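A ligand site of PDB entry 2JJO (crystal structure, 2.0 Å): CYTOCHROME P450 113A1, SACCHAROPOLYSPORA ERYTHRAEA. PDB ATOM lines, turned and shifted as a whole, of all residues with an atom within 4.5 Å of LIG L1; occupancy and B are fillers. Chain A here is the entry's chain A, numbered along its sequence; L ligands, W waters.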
ATOM      1  N   ILE A  87     -37.439  -6.010 -29.350  1.00  0.00           N
ATOM      2  CA  ILE A  87     -37.225  -5.835 -27.912  1.00  0.00           C
ATOM      3  C   ILE A  87     -36.730  -4.411 -27.506  1.00  0.00           C
ATOM      4  O   ILE A  87     -37.220  -3.815 -26.528  1.00  0.00           O
ATOM      5  CB  ILE A  87     -36.290  -6.955 -27.385  1.00  0.00           C
ATOM      6  CG1 ILE A  87     -36.207  -6.950 -25.860  1.00  0.00           C
ATOM      7  CG2 ILE A  87     -34.906  -6.851 -28.048  1.00  0.00           C
ATOM      8  CD1 ILE A  87     -35.257  -8.006 -25.298  1.00  0.00           C
ATOM      9  N   HIS A  88     -35.815  -3.859 -28.298  1.00  0.00           N
ATOM     10  CA  HIS A  88     -35.262  -2.537 -28.054  1.00  0.00           C
ATOM     11  C   HIS A  88     -36.272  -1.392 -28.294  1.00  0.00           C
ATOM     12  O   HIS A  88     -35.937  -0.218 -28.025  1.00  0.00           O
ATOM     13  CB  HIS A  88     -34.012  -2.348 -28.933  1.00  0.00           C
ATOM     14  CG  HIS A  88     -34.331  -2.325 -30.407  1.00  0.00           C
ATOM     15  ND1 HIS A  88     -34.787  -3.442 -31.092  1.00  0.00           N
ATOM     16  CD2 HIS A  88     -34.303  -1.316 -31.313  1.00  0.00           C
ATOM     17  CE1 HIS A  88     -35.033  -3.113 -32.349  1.00  0.00           C
ATOM     18  NE2 HIS A  88     -34.754  -1.831 -32.502  1.00  0.00           N
ATOM     19  N   HIS A  95     -42.184  -5.315 -22.238  1.00  0.00           N
ATOM     20  CA  HIS A  95     -40.718  -5.567 -22.337  1.00  0.00           C
ATOM     21  C   HIS A  95     -40.264  -6.756 -21.499  1.00  0.00           C
ATOM     22  O   HIS A  95     -39.569  -7.631 -22.011  1.00  0.00           O
ATOM     23  CB  HIS A  95     -39.906  -4.322 -21.959  1.00  0.00           C
ATOM     24  CG  HIS A  95     -38.407  -4.537 -21.996  1.00  0.00           C
ATOM     25  ND1 HIS A  95     -37.646  -4.670 -20.845  1.00  0.00           N
ATOM     26  CD2 HIS A  95     -37.544  -4.617 -23.042  1.00  0.00           C
ATOM     27  CE1 HIS A  95     -36.374  -4.821 -21.191  1.00  0.00           C
ATOM     28  NE2 HIS A  95     -36.292  -4.810 -22.507  1.00  0.00           N
ATOM     29  N   ARG A  99     -38.031 -10.010 -22.949  1.00  0.00           N
ATOM     30  CA  ARG A  99     -36.650 -10.141 -22.535  1.00  0.00           C
ATOM     31  C   ARG A  99     -36.422 -11.458 -21.760  1.00  0.00           C
ATOM     32  O   ARG A  99     -35.347 -12.089 -21.886  1.00  0.00           O
ATOM     33  CB  ARG A  99     -36.231  -8.946 -21.671  1.00  0.00           C
ATOM     34  CG  ARG A  99     -34.773  -8.980 -21.312  1.00  0.00           C
ATOM     35  CD  ARG A  99     -34.259  -7.625 -20.890  1.00  0.00           C
ATOM     36  NE  ARG A  99     -32.987  -7.698 -20.173  1.00  0.00           N
ATOM     37  CZ  ARG A  99     -31.989  -6.834 -20.347  1.00  0.00           C
ATOM     38  NH1 ARG A  99     -32.075  -5.838 -21.254  1.00  0.00           N
ATOM     39  NH2 ARG A  99     -30.884  -6.977 -19.596  1.00  0.00           N
ATOM     40  N   PHE A 106     -27.922 -15.410 -21.377  1.00  0.00           N
ATOM     41  CA  PHE A 106     -26.859 -14.412 -21.272  1.00  0.00           C
ATOM     42  C   PHE A 106     -26.311 -14.202 -19.855  1.00  0.00           C
ATOM     43  O   PHE A 106     -25.590 -13.248 -19.628  1.00  0.00           O
ATOM     44  CB  PHE A 106     -27.306 -13.049 -21.815  1.00  0.00           C
ATOM     45  CG  PHE A 106     -27.626 -13.058 -23.275  1.00  0.00           C
ATOM     46  CD1 PHE A 106     -28.925 -13.294 -23.702  1.00  0.00           C
ATOM     47  CD2 PHE A 106     -26.646 -12.786 -24.216  1.00  0.00           C
ATOM     48  CE1 PHE A 106     -29.257 -13.271 -25.073  1.00  0.00           C
ATOM     49  CE2 PHE A 106     -26.959 -12.787 -25.581  1.00  0.00           C
ATOM     50  CZ  PHE A 106     -28.264 -13.015 -26.007  1.00  0.00           C
ATOM     51  N   LEU A 238     -31.478  -9.603 -32.426  1.00  0.00           N
ATOM     52  CA  LEU A 238     -30.430 -10.345 -31.716  1.00  0.00           C
ATOM     53  C   LEU A 238     -29.146 -10.450 -32.575  1.00  0.00           C
ATOM     54  O   LEU A 238     -28.038 -10.283 -32.083  1.00  0.00           O
ATOM     55  CB  LEU A 238     -30.919 -11.732 -31.303  1.00  0.00           C
ATOM     56  CG  LEU A 238     -31.886 -11.732 -30.117  1.00  0.00           C
ATOM     57  CD1 LEU A 238     -32.593 -13.058 -30.034  1.00  0.00           C
ATOM     58  CD2 LEU A 238     -31.143 -11.400 -28.804  1.00  0.00           C
ATOM     59  N   ALA A 241     -27.451  -6.928 -32.861  1.00  0.00           N
ATOM     60  CA  ALA A 241     -26.960  -6.489 -31.562  1.00  0.00           C
ATOM     61  C   ALA A 241     -25.692  -7.256 -31.212  1.00  0.00           C
ATOM     62  O   ALA A 241     -24.829  -6.758 -30.501  1.00  0.00           O
ATOM     63  CB  ALA A 241     -28.005  -6.745 -30.489  1.00  0.00           C
ATOM     64  N   GLY A 242     -25.617  -8.503 -31.705  1.00  0.00           N
ATOM     65  CA  GLY A 242     -24.598  -9.439 -31.296  1.00  0.00           C
ATOM     66  C   GLY A 242     -23.221  -9.247 -31.930  1.00  0.00           C
ATOM     67  O   GLY A 242     -22.262  -9.859 -31.444  1.00  0.00           O
ATOM     68  N   THR A 245     -21.402  -3.776 -32.664  1.00  0.00           N
ATOM     69  CA  THR A 245     -20.737  -2.973 -31.613  1.00  0.00           C
ATOM     70  C   THR A 245     -19.521  -3.682 -30.967  1.00  0.00           C
ATOM     71  O   THR A 245     -18.573  -3.016 -30.531  1.00  0.00           O
ATOM     72  CB  THR A 245     -21.705  -2.616 -30.473  1.00  0.00           C
ATOM     73  OG1 THR A 245     -22.488  -3.787 -30.135  1.00  0.00           O
ATOM     74  CG2 THR A 245     -22.648  -1.533 -30.896  1.00  0.00           C
ATOM     75  N   THR A 246     -19.546  -5.023 -30.923  1.00  0.00           N
ATOM     76  CA  THR A 246     -18.385  -5.776 -30.433  1.00  0.00           C
ATOM     77  C   THR A 246     -17.196  -5.572 -31.344  1.00  0.00           C
ATOM     78  O   THR A 246     -16.063  -5.360 -30.893  1.00  0.00           O
ATOM     79  CB  THR A 246     -18.726  -7.274 -30.281  1.00  0.00           C
ATOM     80  OG1 THR A 246     -19.880  -7.378 -29.438  1.00  0.00           O
ATOM     81  CG2 THR A 246     -17.583  -8.041 -29.632  1.00  0.00           C
ATOM     82  N   LEU A 249     -15.920  -1.996 -30.795  1.00  0.00           N
ATOM     83  CA  LEU A 249     -15.215  -1.808 -29.516  1.00  0.00           C
ATOM     84  C   LEU A 249     -13.800  -2.393 -29.609  1.00  0.00           C
ATOM     85  O   LEU A 249     -12.816  -1.812 -29.118  1.00  0.00           O
ATOM     86  CB  LEU A 249     -15.943  -2.499 -28.363  1.00  0.00           C
ATOM     87  CG  LEU A 249     -15.210  -2.410 -27.001  1.00  0.00           C
ATOM     88  CD1 LEU A 249     -14.996  -0.978 -26.510  1.00  0.00           C
ATOM     89  CD2 LEU A 249     -15.933  -3.244 -25.888  1.00  0.00           C
ATOM     90  N   LEU A 282     -14.742   1.523 -23.434  1.00  0.00           N
ATOM     91  CA  LEU A 282     -16.178   1.730 -23.497  1.00  0.00           C
ATOM     92  C   LEU A 282     -16.590   3.139 -23.094  1.00  0.00           C
ATOM     93  O   LEU A 282     -17.401   3.773 -23.791  1.00  0.00           O
ATOM     94  CB  LEU A 282     -16.932   0.695 -22.656  1.00  0.00           C
ATOM     95  CG  LEU A 282     -17.187  -0.656 -23.378  1.00  0.00           C
ATOM     96  CD1 LEU A 282     -17.379  -1.771 -22.373  1.00  0.00           C
ATOM     97  CD2 LEU A 282     -18.439  -0.603 -24.303  1.00  0.00           C
ATOM     98  N   PRO A 287     -19.103   2.546 -28.657  1.00  0.00           N
ATOM     99  CA  PRO A 287     -19.475   2.136 -30.033  1.00  0.00           C
ATOM    100  C   PRO A 287     -20.786   2.776 -30.557  1.00  0.00           C
ATOM    101  O   PRO A 287     -20.867   3.139 -31.715  1.00  0.00           O
ATOM    102  CB  PRO A 287     -19.639   0.617 -29.894  1.00  0.00           C
ATOM    103  CG  PRO A 287     -18.577   0.264 -28.780  1.00  0.00           C
ATOM    104  CD  PRO A 287     -18.756   1.402 -27.785  1.00  0.00           C
ATOM    105  N   PHE A 288     -21.794   2.882 -29.690  1.00  0.00           N
ATOM    106  CA  PHE A 288     -23.090   3.437 -30.026  1.00  0.00           C
ATOM    107  C   PHE A 288     -23.186   4.720 -29.168  1.00  0.00           C
ATOM    108  O   PHE A 288     -23.503   4.651 -27.974  1.00  0.00           O
ATOM    109  CB  PHE A 288     -24.180   2.417 -29.595  1.00  0.00           C
ATOM    110  CG  PHE A 288     -25.542   2.684 -30.132  1.00  0.00           C
ATOM    111  CD1 PHE A 288     -25.741   2.990 -31.484  1.00  0.00           C
ATOM    112  CD2 PHE A 288     -26.660   2.588 -29.295  1.00  0.00           C
ATOM    113  CE1 PHE A 288     -27.027   3.230 -32.001  1.00  0.00           C
ATOM    114  CE2 PHE A 288     -27.949   2.794 -29.789  1.00  0.00           C
ATOM    115  CZ  PHE A 288     -28.132   3.102 -31.150  1.00  0.00           C
ATOM    116  N   MET A 291     -28.627   7.395 -28.473  1.00  0.00           N
ATOM    117  CA  MET A 291     -29.768   6.527 -28.637  1.00  0.00           C
ATOM    118  C   MET A 291     -31.060   7.336 -28.580  1.00  0.00           C
ATOM    119  O   MET A 291     -31.074   8.417 -27.996  1.00  0.00           O
ATOM    120  CB  MET A 291     -29.839   5.300 -27.689  1.00  0.00           C
ATOM    121  CG  MET A 291     -29.344   5.386 -26.262  1.00  0.00           C
ATOM    122  SD  MET A 291     -28.494   3.787 -25.825  1.00  0.00           S
ATOM    123  CE  MET A 291     -26.833   4.222 -26.232  1.00  0.00           C
ATOM    124  N   ARG A 293     -35.243   8.062 -27.896  1.00  0.00           N
ATOM    125  CA  ARG A 293     -36.478   7.799 -27.175  1.00  0.00           C
ATOM    126  C   ARG A 293     -37.599   8.668 -27.801  1.00  0.00           C
ATOM    127  O   ARG A 293     -37.337   9.524 -28.684  1.00  0.00           O
ATOM    128  CB  ARG A 293     -36.330   8.123 -25.659  1.00  0.00           C
ATOM    129  CG  ARG A 293     -35.297   7.243 -24.878  1.00  0.00           C
ATOM    130  CD  ARG A 293     -35.606   5.748 -25.009  1.00  0.00           C
ATOM    131  NE  ARG A 293     -34.818   4.857 -24.165  1.00  0.00           N
ATOM    132  CZ  ARG A 293     -33.819   4.090 -24.624  1.00  0.00           C
ATOM    133  NH1 ARG A 293     -33.447   4.116 -25.926  1.00  0.00           N
ATOM    134  NH2 ARG A 293     -33.213   3.273 -23.776  1.00  0.00           N
ATOM    135  N   SER A 345     -22.250   2.999 -21.602  1.00  0.00           N
ATOM    136  CA  SER A 345     -22.096   2.602 -23.002  1.00  0.00           C
ATOM    137  C   SER A 345     -22.818   1.313 -23.352  1.00  0.00           C
ATOM    138  O   SER A 345     -22.882   0.938 -24.546  1.00  0.00           O
ATOM    139  CB  SER A 345     -20.615   2.519 -23.380  1.00  0.00           C
ATOM    140  OG  SER A 345     -20.029   3.760 -23.132  1.00  0.00           O
ATOM    141  N   PHE A 346     -23.341   0.630 -22.316  1.00  0.00           N
ATOM    142  CA  PHE A 346     -24.264  -0.496 -22.440  1.00  0.00           C
ATOM    143  C   PHE A 346     -25.728  -0.067 -22.189  1.00  0.00           C
ATOM    144  O   PHE A 346     -26.647  -0.903 -22.147  1.00  0.00           O
ATOM    145  CB  PHE A 346     -23.880  -1.658 -21.488  1.00  0.00           C
ATOM    146  CG  PHE A 346     -22.635  -2.441 -21.922  1.00  0.00           C
ATOM    147  CD1 PHE A 346     -21.599  -2.689 -21.024  1.00  0.00           C
ATOM    148  CD2 PHE A 346     -22.533  -2.976 -23.222  1.00  0.00           C
ATOM    149  CE1 PHE A 346     -20.446  -3.416 -21.412  1.00  0.00           C
ATOM    150  CE2 PHE A 346     -21.394  -3.713 -23.633  1.00  0.00           C
ATOM    151  CZ  PHE A 346     -20.329  -3.920 -22.724  1.00  0.00           C
ATOM    152  N   GLY A 347     -25.936   1.239 -22.022  1.00  0.00           N
ATOM    153  CA  GLY A 347     -27.281   1.734 -21.718  1.00  0.00           C
ATOM    154  C   GLY A 347     -27.463   1.849 -20.218  1.00  0.00           C
ATOM    155  O   GLY A 347     -26.475   1.886 -19.455  1.00  0.00           O
ATOM    156  N   VAL A 350     -33.828  -0.418 -17.791  1.00  0.00           N
ATOM    157  CA  VAL A 350     -34.473  -1.660 -18.229  1.00  0.00           C
ATOM    158  C   VAL A 350     -33.921  -2.265 -19.503  1.00  0.00           C
ATOM    159  O   VAL A 350     -33.967  -3.484 -19.649  1.00  0.00           O
ATOM    160  CB  VAL A 350     -36.023  -1.560 -18.323  1.00  0.00           C
ATOM    161  CG1 VAL A 350     -36.612  -0.752 -17.150  1.00  0.00           C
ATOM    162  CG2 VAL A 350     -36.472  -1.037 -19.655  1.00  0.00           C
ATOM    163  N   HIS A 351     -33.444  -1.432 -20.427  1.00  0.00           N
ATOM    164  CA  HIS A 351     -32.863  -1.952 -21.691  1.00  0.00           C
ATOM    165  C   HIS A 351     -31.334  -2.167 -21.634  1.00  0.00           C
ATOM    166  O   HIS A 351     -30.714  -2.480 -22.624  1.00  0.00           O
ATOM    167  CB  HIS A 351     -33.204  -1.065 -22.875  1.00  0.00           C
ATOM    168  CG  HIS A 351     -34.679  -1.012 -23.189  1.00  0.00           C
ATOM    169  ND1 HIS A 351     -35.297  -1.930 -24.016  1.00  0.00           N
ATOM    170  CD2 HIS A 351     -35.644  -0.159 -22.792  1.00  0.00           C
ATOM    171  CE1 HIS A 351     -36.564  -1.618 -24.137  1.00  0.00           C
ATOM    172  NE2 HIS A 351     -36.815  -0.555 -23.389  1.00  0.00           N
ATOM    173  N   PHE A 352     -30.731  -2.051 -20.449  1.00  0.00           N
ATOM    174  CA  PHE A 352     -29.286  -2.287 -20.321  1.00  0.00           C
ATOM    175  C   PHE A 352     -28.897  -3.550 -21.093  1.00  0.00           C
ATOM    176  O   PHE A 352     -29.512  -4.617 -20.906  1.00  0.00           O
ATOM    177  CB  PHE A 352     -28.898  -2.397 -18.851  1.00  0.00           C
ATOM    178  CG  PHE A 352     -27.391  -2.492 -18.616  1.00  0.00           C
ATOM    179  CD1 PHE A 352     -26.635  -1.330 -18.413  1.00  0.00           C
ATOM    180  CD2 PHE A 352     -26.746  -3.749 -18.600  1.00  0.00           C
ATOM    181  CE1 PHE A 352     -25.269  -1.407 -18.183  1.00  0.00           C
ATOM    182  CE2 PHE A 352     -25.367  -3.840 -18.372  1.00  0.00           C
ATOM    183  CZ  PHE A 352     -24.625  -2.678 -18.171  1.00  0.00           C
ATOM    184  N   CYS A 353     -27.855  -3.402 -21.933  1.00  0.00           N
ATOM    185  CA  CYS A 353     -27.409  -4.445 -22.848  1.00  0.00           C
ATOM    186  C   CYS A 353     -27.462  -5.851 -22.277  1.00  0.00           C
ATOM    187  O   CYS A 353     -26.737  -6.174 -21.313  1.00  0.00           O
ATOM    188  CB  CYS A 353     -25.989  -4.149 -23.333  1.00  0.00           C
ATOM    189  SG  CYS A 353     -25.288  -5.391 -24.449  1.00  0.00           S
ATOM    190  N   LEU A 354     -28.306  -6.688 -22.865  1.00  0.00           N
ATOM    191  CA  LEU A 354     -28.308  -8.129 -22.564  1.00  0.00           C
ATOM    192  C   LEU A 354     -26.964  -8.830 -22.821  1.00  0.00           C
ATOM    193  O   LEU A 354     -26.581  -9.723 -22.076  1.00  0.00           O
ATOM    194  CB  LEU A 354     -29.410  -8.818 -23.384  1.00  0.00           C
ATOM    195  CG  LEU A 354     -30.212 -10.072 -22.994  1.00  0.00           C
ATOM    196  CD1 LEU A 354     -30.628 -10.214 -21.494  1.00  0.00           C
ATOM    197  CD2 LEU A 354     -31.445 -10.083 -23.922  1.00  0.00           C
ATOM    198  N   GLY A 355     -26.263  -8.405 -23.880  1.00  0.00           N
ATOM    199  CA  GLY A 355     -24.995  -9.035 -24.260  1.00  0.00           C
ATOM    200  C   GLY A 355     -23.760  -8.556 -23.517  1.00  0.00           C
ATOM    201  O   GLY A 355     -22.637  -8.967 -23.859  1.00  0.00           O
ATOM    202  N   LEU A 358     -21.062 -10.981 -22.498  1.00  0.00           N
ATOM    203  CA  LEU A 358     -20.507 -11.578 -23.709  1.00  0.00           C
ATOM    204  C   LEU A 358     -19.542 -10.606 -24.436  1.00  0.00           C
ATOM    205  O   LEU A 358     -18.424 -10.977 -24.800  1.00  0.00           O
ATOM    206  CB  LEU A 358     -21.647 -12.076 -24.634  1.00  0.00           C
ATOM    207  CG  LEU A 358     -21.173 -12.725 -25.933  1.00  0.00           C
ATOM    208  CD1 LEU A 358     -20.268 -13.953 -25.636  1.00  0.00           C
ATOM    209  CD2 LEU A 358     -22.347 -13.093 -26.821  1.00  0.00           C
ATOM    210  N   ALA A 359     -19.978  -9.358 -24.625  1.00  0.00           N
ATOM    211  CA  ALA A 359     -19.079  -8.322 -25.179  1.00  0.00           C
ATOM    212  C   ALA A 359     -17.836  -8.147 -24.338  1.00  0.00           C
ATOM    213  O   ALA A 359     -16.715  -8.010 -24.868  1.00  0.00           O
ATOM    214  CB  ALA A 359     -19.822  -6.992 -25.288  1.00  0.00           C
HETATM  215  C1  LIG L   1     -28.980  -3.400 -25.969  1.00  0.00           C
HETATM  216  C2  LIG L   1     -24.511  -1.628 -26.509  1.00  0.00           C
HETATM  217  C3  LIG L   1     -22.900  -6.127 -27.391  1.00  0.00           C
HETATM  218  C4  LIG L   1     -27.424  -7.845 -27.191  1.00  0.00           C
HETATM  219  C5  LIG L   1     -27.899  -2.561 -26.000  1.00  0.00           C
HETATM  220  C6  LIG L   1     -27.955  -1.165 -25.627  1.00  0.00           C
HETATM  221  C7  LIG L   1     -26.734  -0.665 -25.773  1.00  0.00           C
HETATM  222  C8  LIG L   1     -25.863  -1.741 -26.236  1.00  0.00           C
HETATM  223  C9  LIG L   1     -26.263   0.799 -25.514  1.00  0.00           C
HETATM  224  C10 LIG L   1     -29.234  -0.423 -25.132  1.00  0.00           C
HETATM  225  C11 LIG L   1     -30.008   0.286 -26.271  1.00  0.00           C
HETATM  226  C12 LIG L   1     -31.121   1.188 -25.760  1.00  0.00           C
HETATM  227  O1  LIG L   1     -31.162   1.480 -24.509  1.00  0.00           O
HETATM  228  O2  LIG L   1     -31.961   1.676 -26.613  1.00  0.00           O
HETATM  229  C13 LIG L   1     -23.673  -2.709 -26.780  1.00  0.00           C
HETATM  230  C14 LIG L   1     -22.257  -2.619 -26.952  1.00  0.00           C
HETATM  231  C15 LIG L   1     -21.786  -3.853 -27.199  1.00  0.00           C
HETATM  232  C16 LIG L   1     -22.927  -4.779 -27.160  1.00  0.00           C
HETATM  233  C17 LIG L   1     -21.452  -1.280 -26.871  1.00  0.00           C
HETATM  234  C18 LIG L   1     -20.305  -4.246 -27.481  1.00  0.00           C
HETATM  235  C19 LIG L   1     -19.270  -3.605 -26.871  1.00  0.00           C
HETATM  236  C20 LIG L   1     -23.984  -6.985 -27.436  1.00  0.00           C
HETATM  237  C21 LIG L   1     -23.919  -8.410 -27.743  1.00  0.00           C
HETATM  238  C22 LIG L   1     -25.171  -8.889 -27.656  1.00  0.00           C
HETATM  239  C23 LIG L   1     -26.073  -7.778 -27.352  1.00  0.00           C
HETATM  240  C24 LIG L   1     -22.598  -9.186 -28.017  1.00  0.00           C
HETATM  241  C25 LIG L   1     -25.628 -10.342 -27.901  1.00  0.00           C
HETATM  242  C26 LIG L   1     -26.622 -10.580 -28.769  1.00  0.00           C
HETATM  243  C27 LIG L   1     -28.267  -6.820 -26.861  1.00  0.00           C
HETATM  244  C28 LIG L   1     -29.707  -6.920 -26.776  1.00  0.00           C
HETATM  245  C29 LIG L   1     -30.162  -5.539 -26.372  1.00  0.00           C
HETATM  246  C30 LIG L   1     -28.975  -4.739 -26.301  1.00  0.00           C
HETATM  247  C31 LIG L   1     -30.600  -8.183 -26.999  1.00  0.00           C
HETATM  248  C32 LIG L   1     -31.593  -5.032 -26.154  1.00  0.00           C
HETATM  249  C33 LIG L   1     -31.866  -5.171 -24.674  1.00  0.00           C
HETATM  250  C34 LIG L   1     -33.262  -4.715 -24.352  1.00  0.00           C
HETATM  251  O3  LIG L   1     -33.810  -3.832 -25.079  1.00  0.00           O
HETATM  252  O4  LIG L   1     -33.855  -5.207 -23.361  1.00  0.00           O
HETATM  253  N1  LIG L   1     -26.624  -2.892 -26.354  1.00  0.00           N
HETATM  254  N2  LIG L   1     -24.068  -4.044 -26.944  1.00  0.00           N
HETATM  255  N3  LIG L   1     -25.312  -6.629 -27.224  1.00  0.00           N
HETATM  256  N4  LIG L   1     -27.880  -5.523 -26.593  1.00  0.00           N
HETATM  257 FE1  LIG L   1     -25.954  -4.792 -26.579  1.00  0.00          FE
HETATM  258  O1  LG2 L   2     -29.517  -3.579 -33.379  1.00  0.00           O
HETATM  259  C1  LG2 L   2     -30.554  -3.090 -32.901  1.00  0.00           C
HETATM  260  O2  LG2 L   2     -30.693  -2.918 -31.499  1.00  0.00           O
HETATM  261  C2  LG2 L   2     -29.669  -3.425 -30.637  1.00  0.00           C
HETATM  262  C3  LG2 L   2     -30.336  -4.078 -29.430  1.00  0.00           C
HETATM  263  C4  LG2 L   2     -31.387  -5.074 -29.842  1.00  0.00           C
HETATM  264  C5  LG2 L   2     -28.789  -2.255 -30.250  1.00  0.00           C
HETATM  265  C6  LG2 L   2     -29.615  -1.006 -29.983  1.00  0.00           C
HETATM  266  C7  LG2 L   2     -27.716  -1.985 -31.318  1.00  0.00           C
HETATM  267  O3  LG2 L   2     -26.786  -3.077 -31.483  1.00  0.00           O
HETATM  268  C8  LG2 L   2     -26.897  -0.714 -31.057  1.00  0.00           C
HETATM  269  C9  LG2 L   2     -26.074  -0.853 -29.749  1.00  0.00           C
HETATM  270  C10 LG2 L   2     -31.807  -2.642 -33.648  1.00  0.00           C
HETATM  271  C11 LG2 L   2     -32.447  -3.879 -34.269  1.00  0.00           C
HETATM  272  C12 LG2 L   2     -31.530  -1.503 -34.632  1.00  0.00           C
HETATM  273  O4  LG2 L   2     -32.836  -1.014 -35.066  1.00  0.00           O
HETATM  274  C13 LG2 L   2     -33.012  -0.685 -36.422  1.00  0.00           C
HETATM  275  O5  LG2 L   2     -33.268   0.721 -36.481  1.00  0.00           O
HETATM  276  C14 LG2 L   2     -34.483   1.174 -35.891  1.00  0.00           C
HETATM  277  C15 LG2 L   2     -34.550   2.697 -36.066  1.00  0.00           C
HETATM  278  C16 LG2 L   2     -35.625   0.504 -36.627  1.00  0.00           C
HETATM  279  O6  LG2 L   2     -36.880   0.936 -36.075  1.00  0.00           O
HETATM  280  C17 LG2 L   2     -35.546  -1.039 -36.630  1.00  0.00           C
HETATM  281  C18 LG2 L   2     -36.622  -1.583 -37.581  1.00  0.00           C
HETATM  282  O7  LG2 L   2     -35.882  -1.549 -35.338  1.00  0.00           O
HETATM  283  C19 LG2 L   2     -34.145  -1.519 -37.039  1.00  0.00           C
HETATM  284  C20 LG2 L   2     -30.657  -0.373 -34.029  1.00  0.00           C
HETATM  285  C21 LG2 L   2     -31.480   0.587 -33.137  1.00  0.00           C
HETATM  286  C22 LG2 L   2     -29.840   0.340 -35.121  1.00  0.00           C
HETATM  287  C23 LG2 L   2     -28.432  -0.246 -35.347  1.00  0.00           C
HETATM  288  C24 LG2 L   2     -27.861   0.248 -36.678  1.00  0.00           C
HETATM  289  O8  LG2 L   2     -28.520  -1.691 -35.484  1.00  0.00           O
HETATM  290  C25 LG2 L   2     -27.549   0.229 -34.168  1.00  0.00           C
HETATM  291  C26 LG2 L   2     -26.420  -0.679 -33.695  1.00  0.00           C
HETATM  292  C27 LG2 L   2     -25.203  -0.556 -34.631  1.00  0.00           C
HETATM  293  C28 LG2 L   2     -26.019  -0.402 -32.273  1.00  0.00           C
HETATM  294  O9  LG2 L   2     -24.920   0.052 -32.069  1.00  0.00           O
HETATM  295  O10 LG2 L   2     -29.642   1.718 -34.848  1.00  0.00           O
HETATM  296  C29 LG2 L   2     -30.433   2.598 -35.643  1.00  0.00           C
HETATM  297  O11 LG2 L   2     -30.101   2.514 -37.034  1.00  0.00           O
HETATM  298  C30 LG2 L   2     -30.921   3.367 -37.837  1.00  0.00           C
HETATM  299  C31 LG2 L   2     -30.584   3.113 -39.275  1.00  0.00           C
HETATM  300  C32 LG2 L   2     -30.735   4.842 -37.441  1.00  0.00           C
HETATM  301  C33 LG2 L   2     -30.945   5.025 -35.918  1.00  0.00           C
HETATM  302  N1  LG2 L   2     -30.714   6.395 -35.378  1.00  0.00           N
HETATM  303  C34 LG2 L   2     -31.702   7.330 -35.949  1.00  0.00           C
HETATM  304  C35 LG2 L   2     -29.349   6.953 -35.532  1.00  0.00           C
HETATM  305  C36 LG2 L   2     -30.098   4.007 -35.159  1.00  0.00           C
HETATM  306  O12 LG2 L   2     -30.374   4.115 -33.749  1.00  0.00           O
HETATM  307  O   HOH W   1     -22.178  -6.372 -30.678  1.00  0.00           O
HETATM  308  O   HOH W   2     -32.015   1.902 -29.194  1.00  0.00           O
HETATM  309  O   HOH W   3     -34.535   0.775 -25.970  1.00  0.00           O
HETATM  310  O   HOH W   4     -25.578  -4.282 -29.099  1.00  0.00           O
HETATM  311  O   HOH W   5     -30.561   1.561 -21.814  1.00  0.00           O
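Water W4 lies within hydrogen-bond range of an oxygen (O3) of LG2 L2 (2.9 Å), the backbone carbonyl oxygen of Ala 241 (2.9 Å) and the side-chain hydroxyl of Thr 245 (3.3 Å).
Water W3 lies within hydrogen-bond range of the backbone carbonyl oxygen of His 88 (2.7 Å), an oxygen (O2) of LIG L1 (2.8 Å) and a ring nitrogen (ND1) of His 351 (3.4 Å).
Water W1 lies within hydrogen-bond range of the side-chain hydroxyl of Thr 245 (2.7 Å), the backbone carbonyl oxygen of Ala 241 (2.7 Å) and the side-chain hydroxyl of Thr 246 (2.8 Å).
SG of Cys 353 is bound to FE1 of LIG L1 (2.3 Å).
An oxygen (O4) of LIG L1 lies within salt-bridge range of the guanidinium group (NH1) of Arg 99, at 2.8 Å.
A ring nitrogen (NE2) of His 95 sits at hydrogen-bond distance from an oxygen (O4) of LIG L1 (2.6 Å).
The guanidinium group (NH2) of Arg 293 lies within salt-bridge range of an oxygen (O1) of LIG L1 (2.8 Å).
A ring nitrogen (NE2) of His 88 is in hydrogen-bond range of an oxygen (O7) of LG2 L2 (3.1 Å).
O3 of LIG L1 lies within hydrogen-bond range of ND1 of His 351.
N of Cys 353 lies within hydrogen-bond range of O of Phe 346, at 2.8 Å.
NH1 of Arg 99 lies within hydrogen-bond range of O of Val 350 (3.4 Å).
N of Gly 355 sits close to SG of Cys 353, 3.2 Å away.
O of Phe 352 lies within hydrogen-bond range of NH1 of Arg 99.
A ring nitrogen (NE2) of His 95 lies within hydrogen-bond range of a ring nitrogen (ND1) of His 351 (3.4 Å).
The side-chain hydroxyl (OG) of Ser 345 sits at hydrogen-bond distance from the backbone carbonyl oxygen (O) of Leu 282 (2.7 Å).
O of Ala 241 sits close to N3 of LIG L1, at 3.3 Å.
O1 of LIG L1 lies close to SD of Met 291 (3.8 Å).
Residues that only touch LIG L1: Ile 87 (3.7 Å), His 88 (3.6 Å), Phe 106 (3.6 Å), Leu 238 (3.6 Å), Gly 242 (3.4 Å), Thr 245 (3.0 Å), Thr 246 (3.6 Å), Leu 249 (3.5 Å), Pro 287 (3.8 Å), Ser 345 (3.5 Å), Phe 346 (3.5 Å), Gly 347 (3.5 Å), Leu 354 (3.7 Å), Gly 355 (3.4 Å) and Ala 359 (3.5 Å).
Hydrophobic or aromatic side chains within 4 Å of LIG L1: Ile 87, His 95, Phe 106, Leu 238, Ala 241, Leu 249, Pro 287, Met 291, Phe 346, His 351, Leu 354 and Ala 359.
Of the 27 residues printed, 22 come within 4 Å of LIG L1.
The nearest printed residue that does not touch LIG L1 is Leu 282 (4.02 Å).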
